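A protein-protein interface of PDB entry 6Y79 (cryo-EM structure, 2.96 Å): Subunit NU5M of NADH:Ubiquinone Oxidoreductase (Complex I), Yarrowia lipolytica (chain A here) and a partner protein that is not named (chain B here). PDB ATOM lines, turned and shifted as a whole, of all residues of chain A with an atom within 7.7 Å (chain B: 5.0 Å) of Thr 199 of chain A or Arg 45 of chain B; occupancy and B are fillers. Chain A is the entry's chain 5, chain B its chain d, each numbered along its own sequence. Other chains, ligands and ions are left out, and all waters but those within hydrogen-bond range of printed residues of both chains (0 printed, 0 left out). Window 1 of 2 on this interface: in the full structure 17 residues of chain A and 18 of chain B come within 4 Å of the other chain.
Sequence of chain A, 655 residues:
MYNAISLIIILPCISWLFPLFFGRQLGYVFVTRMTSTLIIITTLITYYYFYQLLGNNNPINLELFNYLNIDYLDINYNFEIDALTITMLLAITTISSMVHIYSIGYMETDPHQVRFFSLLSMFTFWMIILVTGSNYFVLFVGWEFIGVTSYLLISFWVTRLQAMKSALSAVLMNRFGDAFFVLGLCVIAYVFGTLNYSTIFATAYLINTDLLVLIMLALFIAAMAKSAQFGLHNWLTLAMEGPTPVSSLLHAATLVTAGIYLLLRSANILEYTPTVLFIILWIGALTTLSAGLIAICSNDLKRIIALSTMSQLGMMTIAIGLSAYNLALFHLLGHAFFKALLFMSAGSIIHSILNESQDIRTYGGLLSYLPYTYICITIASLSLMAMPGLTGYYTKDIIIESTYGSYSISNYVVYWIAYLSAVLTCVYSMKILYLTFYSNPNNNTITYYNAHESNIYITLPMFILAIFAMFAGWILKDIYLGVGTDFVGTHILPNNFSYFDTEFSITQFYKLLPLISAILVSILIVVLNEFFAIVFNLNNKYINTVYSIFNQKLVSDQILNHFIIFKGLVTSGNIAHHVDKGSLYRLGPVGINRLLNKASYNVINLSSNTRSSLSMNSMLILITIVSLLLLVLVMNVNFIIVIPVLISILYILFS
The side-chain hydroxyl (OH) of Tyr 70 of chain B is in hydrogen-bond range of the backbone carbonyl oxygen (O) of Phe 192 of chain A, at 2.9 Å. NH2 of Arg 45 of chain B sits at hydrogen-bond distance from O of Tyr 72 of chain A, 3.2 Å away. NZ of Lys 42 of chain B sits at hydrogen-bond distance from OD1 of Asn 69 of chain A (2.4 Å). OG1 of Thr 199 of chain A lies within hydrogen-bond range of OE1 of Glu 49 of chain B (3.4 Å).
O of Thr 199 of chain A sits at hydrogen-bond distance from OG1 of Thr 203 of chain A.
Ile 70 of chain A touches Lys 42 of chain B (O to NZ, 3.9 Å). Asp 71 of chain A touches Lys 42 of chain B (O to CE, 3.3 Å). OH of Tyr 70 of chain B touches O of Gly 193 of chain A, 3.8 Å away. Ser 198 of chain A touches Glu 49 of chain B (CB to CB, 3.9 Å). Arg 45 of chain B touches Thr 199 of chain A. CG2 of Thr 203 of chain A touches CD2 of Leu 48 of chain B, at 3.7 Å.
Of chain B, only Arg 45 (3.8 Å) and Glu 49 (3.4 Å) come within 4 Å of Thr 199 of chain A. Of the printed residues of chain A, Arg 45 of chain B touches Tyr 72 (3.2 Å) and Thr 199 (3.8 Å). Of the printed residues of chain B, Ser 198 of chain A touches Glu 49. Of the printed residues of chain A, Leu 48 of chain B touches Thr 203 (3.7 Å). Printed residues of chain B within 4 Å of Asp 71 of chain A: Lys 42. Ile 75 of chain A touches none of the printed residues of chain B. Ala 204 of chain A touches none of the printed residues of chain B.
Of the 21 printed residues of chain A, 9 touch a printed residue of chain B. Hydrophobic or aromatic side chains of chain B within 4 Å of the printed part of chain A: Leu 48 and Tyr 70.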
ATOM      1  N   ASN A  69     -13.753  16.275   5.585  1.00  0.00           N
ATOM      2  CA  ASN A  69     -14.898  15.903   6.400  1.00  0.00           C
ATOM      3  C   ASN A  69     -15.708  17.158   6.676  1.00  0.00           C
ATOM      4  O   ASN A  69     -15.341  17.961   7.535  1.00  0.00           O
ATOM      5  CB  ASN A  69     -14.452  15.272   7.712  1.00  0.00           C
ATOM      6  CG  ASN A  69     -15.555  14.542   8.408  1.00  0.00           C
ATOM      7  OD1 ASN A  69     -16.669  14.443   7.902  1.00  0.00           O
ATOM      8  ND2 ASN A  69     -15.258  14.022   9.587  1.00  0.00           N
ATOM      9  N   ILE A  70     -16.815  17.301   5.966  1.00  0.00           N
ATOM     10  CA  ILE A  70     -17.791  18.370   6.126  1.00  0.00           C
ATOM     11  C   ILE A  70     -18.989  17.534   6.543  1.00  0.00           C
ATOM     12  O   ILE A  70     -18.789  16.357   6.859  1.00  0.00           O
ATOM     13  CB  ILE A  70     -17.961  19.204   4.838  1.00  0.00           C
ATOM     14  CG1 ILE A  70     -16.590  19.695   4.396  1.00  0.00           C
ATOM     15  CG2 ILE A  70     -18.743  20.504   5.044  1.00  0.00           C
ATOM     16  CD1 ILE A  70     -15.859  20.483   5.470  1.00  0.00           C
ATOM     17  N   ASP A  71     -20.190  18.115   6.650  1.00  0.00           N
ATOM     18  CA  ASP A  71     -21.248  17.534   7.467  1.00  0.00           C
ATOM     19  C   ASP A  71     -21.688  16.132   7.052  1.00  0.00           C
ATOM     20  O   ASP A  71     -21.308  15.165   7.714  1.00  0.00           O
ATOM     21  CB  ASP A  71     -22.464  18.470   7.521  1.00  0.00           C
ATOM     22  CG  ASP A  71     -22.891  18.985   6.165  1.00  0.00           C
ATOM     23  OD1 ASP A  71     -22.153  18.758   5.191  1.00  0.00           O
ATOM     24  OD2 ASP A  71     -23.979  19.588   6.071  1.00  0.00           O
ATOM     25  N   TYR A  72     -22.353  15.964   5.923  1.00  0.00           N
ATOM     26  CA  TYR A  72     -22.794  14.637   5.542  1.00  0.00           C
ATOM     27  C   TYR A  72     -21.833  13.971   4.577  1.00  0.00           C
ATOM     28  O   TYR A  72     -22.118  12.874   4.098  1.00  0.00           O
ATOM     29  CB  TYR A  72     -24.208  14.698   4.960  1.00  0.00           C
ATOM     30  CG  TYR A  72     -24.355  15.466   3.671  1.00  0.00           C
ATOM     31  CD1 TYR A  72     -24.624  16.827   3.669  1.00  0.00           C
ATOM     32  CD2 TYR A  72     -24.267  14.822   2.453  1.00  0.00           C
ATOM     33  CE1 TYR A  72     -24.774  17.522   2.483  1.00  0.00           C
ATOM     34  CE2 TYR A  72     -24.407  15.502   1.273  1.00  0.00           C
ATOM     35  CZ  TYR A  72     -24.664  16.847   1.286  1.00  0.00           C
ATOM     36  OH  TYR A  72     -24.808  17.495   0.086  1.00  0.00           O
ATOM     37  N   LEU A  73     -20.689  14.593   4.310  1.00  0.00           N
ATOM     38  CA  LEU A  73     -19.839  14.233   3.184  1.00  0.00           C
ATOM     39  C   LEU A  73     -18.408  14.045   3.649  1.00  0.00           C
ATOM     40  O   LEU A  73     -17.771  15.001   4.093  1.00  0.00           O
ATOM     41  CB  LEU A  73     -19.896  15.313   2.107  1.00  0.00           C
ATOM     42  CG  LEU A  73     -19.072  15.058   0.852  1.00  0.00           C
ATOM     43  CD1 LEU A  73     -19.606  13.846   0.128  1.00  0.00           C
ATOM     44  CD2 LEU A  73     -19.097  16.270  -0.047  1.00  0.00           C
ATOM     45  N   ASP A  74     -17.898  12.823   3.529  1.00  0.00           N
ATOM     46  CA  ASP A  74     -16.486  12.546   3.728  1.00  0.00           C
ATOM     47  C   ASP A  74     -15.896  12.017   2.430  1.00  0.00           C
ATOM     48  O   ASP A  74     -16.538  11.279   1.679  1.00  0.00           O
ATOM     49  CB  ASP A  74     -16.245  11.539   4.864  1.00  0.00           C
ATOM     50  CG  ASP A  74     -14.790  11.523   5.362  1.00  0.00           C
ATOM     51  OD1 ASP A  74     -13.859  11.877   4.609  1.00  0.00           O
ATOM     52  OD2 ASP A  74     -14.569  11.136   6.529  1.00  0.00           O
ATOM     53  N   ILE A  75     -14.651  12.416   2.186  1.00  0.00           N
ATOM     54  CA  ILE A  75     -13.848  11.959   1.063  1.00  0.00           C
ATOM     55  C   ILE A  75     -12.509  11.531   1.637  1.00  0.00           C
ATOM     56  O   ILE A  75     -11.894  12.280   2.402  1.00  0.00           O
ATOM     57  CB  ILE A  75     -13.664  13.057   0.000  1.00  0.00           C
ATOM     58  CG1 ILE A  75     -15.004  13.425  -0.638  1.00  0.00           C
ATOM     59  CG2 ILE A  75     -12.690  12.622  -1.063  1.00  0.00           C
ATOM     60  CD1 ILE A  75     -14.989  14.728  -1.370  1.00  0.00           C
ATOM     61  N   ASN A  76     -12.076  10.323   1.311  1.00  0.00           N
ATOM     62  CA  ASN A  76     -10.778   9.835   1.741  1.00  0.00           C
ATOM     63  C   ASN A  76      -9.955   9.438   0.527  1.00  0.00           C
ATOM     64  O   ASN A  76     -10.499   9.074  -0.517  1.00  0.00           O
ATOM     65  CB  ASN A  76     -10.912   8.635   2.683  1.00  0.00           C
ATOM     66  CG  ASN A  76     -11.480   9.002   4.039  1.00  0.00           C
ATOM     67  OD1 ASN A  76     -11.076   9.985   4.652  1.00  0.00           O
ATOM     68  ND2 ASN A  76     -12.416   8.199   4.519  1.00  0.00           N
ATOM     69  N   PHE A 192     -26.614  10.819  -3.043  1.00  0.00           N
ATOM     70  CA  PHE A 192     -26.143   9.748  -2.184  1.00  0.00           C
ATOM     71  C   PHE A 192     -25.465  10.255  -0.929  1.00  0.00           C
ATOM     72  O   PHE A 192     -25.327   9.495   0.033  1.00  0.00           O
ATOM     73  CB  PHE A 192     -25.179   8.846  -2.950  1.00  0.00           C
ATOM     74  CG  PHE A 192     -25.824   8.103  -4.073  1.00  0.00           C
ATOM     75  CD1 PHE A 192     -26.413   6.875  -3.852  1.00  0.00           C
ATOM     76  CD2 PHE A 192     -25.859   8.640  -5.345  1.00  0.00           C
ATOM     77  CE1 PHE A 192     -27.013   6.195  -4.881  1.00  0.00           C
ATOM     78  CE2 PHE A 192     -26.463   7.964  -6.377  1.00  0.00           C
ATOM     79  CZ  PHE A 192     -27.041   6.739  -6.144  1.00  0.00           C
ATOM     80  N   GLY A 193     -25.040  11.511  -0.912  1.00  0.00           N
ATOM     81  CA  GLY A 193     -24.348  12.038   0.238  1.00  0.00           C
ATOM     82  C   GLY A 193     -22.936  11.544   0.409  1.00  0.00           C
ATOM     83  O   GLY A 193     -22.362  11.716   1.484  1.00  0.00           O
ATOM     84  N   THR A 194     -22.362  10.931  -0.616  1.00  0.00           N
ATOM     85  CA  THR A 194     -21.031  10.359  -0.538  1.00  0.00           C
ATOM     86  C   THR A 194     -20.492  10.238  -1.950  1.00  0.00           C
ATOM     87  O   THR A 194     -21.208  10.450  -2.931  1.00  0.00           O
ATOM     88  CB  THR A 194     -21.043   8.992   0.145  1.00  0.00           C
ATOM     89  OG1 THR A 194     -19.699   8.561   0.384  1.00  0.00           O
ATOM     90  CG2 THR A 194     -21.743   7.986  -0.731  1.00  0.00           C
ATOM     91  N   LEU A 195     -19.215   9.894  -2.044  1.00  0.00           N
ATOM     92  CA  LEU A 195     -18.588   9.629  -3.323  1.00  0.00           C
ATOM     93  C   LEU A 195     -18.055   8.212  -3.417  1.00  0.00           C
ATOM     94  O   LEU A 195     -17.600   7.814  -4.491  1.00  0.00           O
ATOM     95  CB  LEU A 195     -17.457  10.633  -3.583  1.00  0.00           C
ATOM     96  CG  LEU A 195     -17.818  11.961  -4.252  1.00  0.00           C
ATOM     97  CD1 LEU A 195     -18.449  12.910  -3.295  1.00  0.00           C
ATOM     98  CD2 LEU A 195     -16.594  12.601  -4.809  1.00  0.00           C
ATOM     99  N   ASN A 196     -18.122   7.438  -2.336  1.00  0.00           N
ATOM    100  CA  ASN A 196     -17.517   6.114  -2.286  1.00  0.00           C
ATOM    101  C   ASN A 196     -18.301   5.137  -3.148  1.00  0.00           C
ATOM    102  O   ASN A 196     -19.529   5.187  -3.177  1.00  0.00           O
ATOM    103  CB  ASN A 196     -17.472   5.620  -0.845  1.00  0.00           C
ATOM    104  CG  ASN A 196     -16.565   6.456   0.029  1.00  0.00           C
ATOM    105  OD1 ASN A 196     -15.494   6.882  -0.394  1.00  0.00           O
ATOM    106  ND2 ASN A 196     -16.987   6.689   1.261  1.00  0.00           N
ATOM    107  N   TYR A 197     -17.583   4.251  -3.851  1.00  0.00           N
ATOM    108  CA  TYR A 197     -18.230   3.304  -4.756  1.00  0.00           C
ATOM    109  C   TYR A 197     -19.116   2.326  -4.000  1.00  0.00           C
ATOM    110  O   TYR A 197     -20.179   1.935  -4.495  1.00  0.00           O
ATOM    111  CB  TYR A 197     -17.194   2.509  -5.550  1.00  0.00           C
ATOM    112  CG  TYR A 197     -16.391   3.255  -6.594  1.00  0.00           C
ATOM    113  CD1 TYR A 197     -16.945   3.654  -7.796  1.00  0.00           C
ATOM    114  CD2 TYR A 197     -15.059   3.491  -6.403  1.00  0.00           C
ATOM    115  CE1 TYR A 197     -16.174   4.301  -8.747  1.00  0.00           C
ATOM    116  CE2 TYR A 197     -14.301   4.143  -7.346  1.00  0.00           C
ATOM    117  CZ  TYR A 197     -14.855   4.552  -8.499  1.00  0.00           C
ATOM    118  OH  TYR A 197     -14.059   5.196  -9.410  1.00  0.00           O
ATOM    119  N   SER A 198     -18.694   1.927  -2.799  1.00  0.00           N
ATOM    120  CA  SER A 198     -19.403   0.896  -2.048  1.00  0.00           C
ATOM    121  C   SER A 198     -20.769   1.384  -1.583  1.00  0.00           C
ATOM    122  O   SER A 198     -21.773   0.676  -1.726  1.00  0.00           O
ATOM    123  CB  SER A 198     -18.558   0.453  -0.858  1.00  0.00           C
ATOM    124  OG  SER A 198     -17.220   0.218  -1.251  1.00  0.00           O
ATOM    125  N   THR A 199     -20.829   2.605  -1.052  1.00  0.00           N
ATOM    126  CA  THR A 199     -22.098   3.141  -0.580  1.00  0.00           C
ATOM    127  C   THR A 199     -23.024   3.463  -1.746  1.00  0.00           C
ATOM    128  O   THR A 199     -24.233   3.219  -1.670  1.00  0.00           O
ATOM    129  CB  THR A 199     -21.846   4.378   0.280  1.00  0.00           C
ATOM    130  OG1 THR A 199     -20.975   4.028   1.362  1.00  0.00           O
ATOM    131  CG2 THR A 199     -23.149   4.921   0.859  1.00  0.00           C
ATOM    132  N   ILE A 200     -22.468   3.977  -2.844  1.00  0.00           N
ATOM    133  CA  ILE A 200     -23.283   4.347  -3.995  1.00  0.00           C
ATOM    134  C   ILE A 200     -23.853   3.110  -4.675  1.00  0.00           C
ATOM    135  O   ILE A 200     -25.023   3.090  -5.068  1.00  0.00           O
ATOM    136  CB  ILE A 200     -22.461   5.219  -4.962  1.00  0.00           C
ATOM    137  CG1 ILE A 200     -22.208   6.583  -4.340  1.00  0.00           C
ATOM    138  CG2 ILE A 200     -23.178   5.449  -6.260  1.00  0.00           C
ATOM    139  CD1 ILE A 200     -21.159   7.352  -5.046  1.00  0.00           C
ATOM    140  N   PHE A 201     -23.071   2.038  -4.769  1.00  0.00           N
ATOM    141  CA  PHE A 201     -23.586   0.834  -5.409  1.00  0.00           C
ATOM    142  C   PHE A 201     -24.449   0.005  -4.472  1.00  0.00           C
ATOM    143  O   PHE A 201     -25.258  -0.795  -4.945  1.00  0.00           O
ATOM    144  CB  PHE A 201     -22.443  -0.028  -5.949  1.00  0.00           C
ATOM    145  CG  PHE A 201     -21.613   0.648  -7.003  1.00  0.00           C
ATOM    146  CD1 PHE A 201     -22.146   1.654  -7.795  1.00  0.00           C
ATOM    147  CD2 PHE A 201     -20.292   0.284  -7.191  1.00  0.00           C
ATOM    148  CE1 PHE A 201     -21.377   2.281  -8.742  1.00  0.00           C
ATOM    149  CE2 PHE A 201     -19.521   0.910  -8.139  1.00  0.00           C
ATOM    150  CZ  PHE A 201     -20.066   1.908  -8.911  1.00  0.00           C
ATOM    151  N   ALA A 202     -24.297   0.178  -3.158  1.00  0.00           N
ATOM    152  CA  ALA A 202     -25.185  -0.500  -2.223  1.00  0.00           C
ATOM    153  C   ALA A 202     -26.586   0.094  -2.244  1.00  0.00           C
ATOM    154  O   ALA A 202     -27.558  -0.612  -1.963  1.00  0.00           O
ATOM    155  CB  ALA A 202     -24.606  -0.435  -0.812  1.00  0.00           C
ATOM    156  N   THR A 203     -26.712   1.376  -2.577  1.00  0.00           N
ATOM    157  CA  THR A 203     -27.986   2.081  -2.535  1.00  0.00           C
ATOM    158  C   THR A 203     -28.458   2.533  -3.907  1.00  0.00           C
ATOM    159  O   THR A 203     -29.332   3.395  -3.992  1.00  0.00           O
ATOM    160  CB  THR A 203     -27.891   3.296  -1.614  1.00  0.00           C
ATOM    161  OG1 THR A 203     -26.822   4.143  -2.048  1.00  0.00           O
ATOM    162  CG2 THR A 203     -27.640   2.874  -0.197  1.00  0.00           C
ATOM    163  N   ALA A 204     -27.899   1.983  -4.983  1.00  0.00           N
ATOM    164  CA  ALA A 204     -28.216   2.497  -6.311  1.00  0.00           C
ATOM    165  C   ALA A 204     -29.587   2.059  -6.796  1.00  0.00           C
ATOM    166  O   ALA A 204     -30.268   2.829  -7.477  1.00  0.00           O
ATOM    167  CB  ALA A 204     -27.162   2.056  -7.323  1.00  0.00           C
ATOM    168  N   LEU B  41     -25.488   9.180  11.585  1.00  0.00           N
ATOM    169  CA  LEU B  41     -25.650   8.913  10.150  1.00  0.00           C
ATOM    170  C   LEU B  41     -24.391   8.294   9.534  1.00  0.00           C
ATOM    171  O   LEU B  41     -24.469   7.356   8.725  1.00  0.00           O
ATOM    172  CB  LEU B  41     -26.017  10.205   9.424  1.00  0.00           C
ATOM    173  CG  LEU B  41     -25.947  10.195   7.901  1.00  0.00           C
ATOM    174  CD1 LEU B  41     -27.056   9.349   7.336  1.00  0.00           C
ATOM    175  CD2 LEU B  41     -26.013  11.593   7.345  1.00  0.00           C
ATOM    176  N   LYS B  42     -23.216   8.793   9.927  1.00  0.00           N
ATOM    177  CA  LYS B  42     -21.961   8.251   9.403  1.00  0.00           C
ATOM    178  C   LYS B  42     -21.696   6.829   9.886  1.00  0.00           C
ATOM    179  O   LYS B  42     -21.118   6.021   9.143  1.00  0.00           O
ATOM    180  CB  LYS B  42     -20.793   9.142   9.797  1.00  0.00           C
ATOM    181  CG  LYS B  42     -20.794  10.490   9.135  1.00  0.00           C
ATOM    182  CD  LYS B  42     -19.579  11.271   9.561  1.00  0.00           C
ATOM    183  CE  LYS B  42     -19.575  12.637   8.939  1.00  0.00           C
ATOM    184  NZ  LYS B  42     -18.357  13.383   9.317  1.00  0.00           N
ATOM    185  N   THR B  43     -22.094   6.518  11.125  1.00  0.00           N
ATOM    186  CA  THR B  43     -21.983   5.158  11.644  1.00  0.00           C
ATOM    187  C   THR B  43     -22.809   4.187  10.815  1.00  0.00           C
ATOM    188  O   THR B  43     -22.330   3.100  10.455  1.00  0.00           O
ATOM    189  CB  THR B  43     -22.426   5.131  13.107  1.00  0.00           C
ATOM    190  OG1 THR B  43     -21.557   5.964  13.883  1.00  0.00           O
ATOM    191  CG2 THR B  43     -22.395   3.719  13.666  1.00  0.00           C
ATOM    192  N   VAL B  44     -24.034   4.583  10.462  1.00  0.00           N
ATOM    193  CA  VAL B  44     -24.850   3.699   9.630  1.00  0.00           C
ATOM    194  C   VAL B  44     -24.281   3.573   8.216  1.00  0.00           C
ATOM    195  O   VAL B  44     -24.348   2.494   7.614  1.00  0.00           O
ATOM    196  CB  VAL B  44     -26.306   4.181   9.624  1.00  0.00           C
ATOM    197  CG1 VAL B  44     -27.201   3.250   8.821  1.00  0.00           C
ATOM    198  CG2 VAL B  44     -26.814   4.273  11.037  1.00  0.00           C
ATOM    199  N   ARG B  45     -23.664   4.636   7.684  1.00  0.00           N
ATOM    200  CA  ARG B  45     -23.042   4.544   6.358  1.00  0.00           C
ATOM    201  C   ARG B  45     -21.866   3.567   6.338  1.00  0.00           C
ATOM    202  O   ARG B  45     -21.737   2.759   5.407  1.00  0.00           O
ATOM    203  CB  ARG B  45     -22.578   5.921   5.896  1.00  0.00           C
ATOM    204  CG  ARG B  45     -22.106   5.956   4.463  1.00  0.00           C
ATOM    205  CD  ARG B  45     -21.781   7.363   4.013  1.00  0.00           C
ATOM    206  NE  ARG B  45     -20.639   7.923   4.723  1.00  0.00           N
ATOM    207  CZ  ARG B  45     -20.635   9.114   5.309  1.00  0.00           C
ATOM    208  NH1 ARG B  45     -19.548   9.539   5.935  1.00  0.00           N
ATOM    209  NH2 ARG B  45     -21.711   9.880   5.258  1.00  0.00           N
ATOM    210  N   LYS B  46     -21.005   3.622   7.359  1.00  0.00           N
ATOM    211  CA  LYS B  46     -19.877   2.693   7.410  1.00  0.00           C
ATOM    212  C   LYS B  46     -20.347   1.259   7.635  1.00  0.00           C
ATOM    213  O   LYS B  46     -19.780   0.315   7.068  1.00  0.00           O
ATOM    214  CB  LYS B  46     -18.891   3.111   8.498  1.00  0.00           C
ATOM    215  CG  LYS B  46     -17.596   2.329   8.482  1.00  0.00           C
ATOM    216  CD  LYS B  46     -16.811   2.526   9.764  1.00  0.00           C
ATOM    217  CE  LYS B  46     -17.086   1.408  10.753  1.00  0.00           C
ATOM    218  NZ  LYS B  46     -15.900   1.099  11.591  1.00  0.00           N
ATOM    219  N   ALA B  47     -21.411   1.082   8.428  1.00  0.00           N
ATOM    220  CA  ALA B  47     -22.002  -0.242   8.601  1.00  0.00           C
ATOM    221  C   ALA B  47     -22.575  -0.774   7.293  1.00  0.00           C
ATOM    222  O   ALA B  47     -22.461  -1.967   6.995  1.00  0.00           O
ATOM    223  CB  ALA B  47     -23.091  -0.189   9.669  1.00  0.00           C
ATOM    224  N   LEU B  48     -23.165   0.106   6.485  1.00  0.00           N
ATOM    225  CA  LEU B  48     -23.747  -0.317   5.217  1.00  0.00           C
ATOM    226  C   LEU B  48     -22.677  -0.711   4.210  1.00  0.00           C
ATOM    227  O   LEU B  48     -22.851  -1.680   3.463  1.00  0.00           O
ATOM    228  CB  LEU B  48     -24.617   0.798   4.653  1.00  0.00           C
ATOM    229  CG  LEU B  48     -25.127   0.670   3.225  1.00  0.00           C
ATOM    230  CD1 LEU B  48     -26.049  -0.521   3.075  1.00  0.00           C
ATOM    231  CD2 LEU B  48     -25.831   1.943   2.873  1.00  0.00           C
ATOM    232  N   GLU B  49     -21.564   0.020   4.161  1.00  0.00           N
ATOM    233  CA  GLU B  49     -20.530  -0.370   3.207  1.00  0.00           C
ATOM    234  C   GLU B  49     -19.767  -1.594   3.692  1.00  0.00           C
ATOM    235  O   GLU B  49     -19.260  -2.370   2.877  1.00  0.00           O
ATOM    236  CB  GLU B  49     -19.586   0.787   2.903  1.00  0.00           C
ATOM    237  CG  GLU B  49     -18.709   1.248   4.022  1.00  0.00           C
ATOM    238  CD  GLU B  49     -17.862   2.428   3.600  1.00  0.00           C
ATOM    239  OE1 GLU B  49     -17.985   2.859   2.431  1.00  0.00           O
ATOM    240  OE2 GLU B  49     -17.081   2.930   4.434  1.00  0.00           O
ATOM    241  N   TYR B  70     -30.194   4.280   5.606  1.00  0.00           N
ATOM    242  CA  TYR B  70     -29.286   5.350   5.198  1.00  0.00           C
ATOM    243  C   TYR B  70     -29.990   6.358   4.304  1.00  0.00           C
ATOM    244  O   TYR B  70     -29.835   7.570   4.477  1.00  0.00           O
ATOM    245  CB  TYR B  70     -28.059   4.790   4.482  1.00  0.00           C
ATOM    246  CG  TYR B  70     -27.114   5.878   4.013  1.00  0.00           C
ATOM    247  CD1 TYR B  70     -26.297   6.537   4.912  1.00  0.00           C
ATOM    248  CD2 TYR B  70     -27.055   6.258   2.676  1.00  0.00           C
ATOM    249  CE1 TYR B  70     -25.448   7.536   4.500  1.00  0.00           C
ATOM    250  CE2 TYR B  70     -26.208   7.260   2.256  1.00  0.00           C
ATOM    251  CZ  TYR B  70     -25.404   7.891   3.174  1.00  0.00           C
ATOM    252  OH  TYR B  70     -24.550   8.885   2.767  1.00  0.00           O
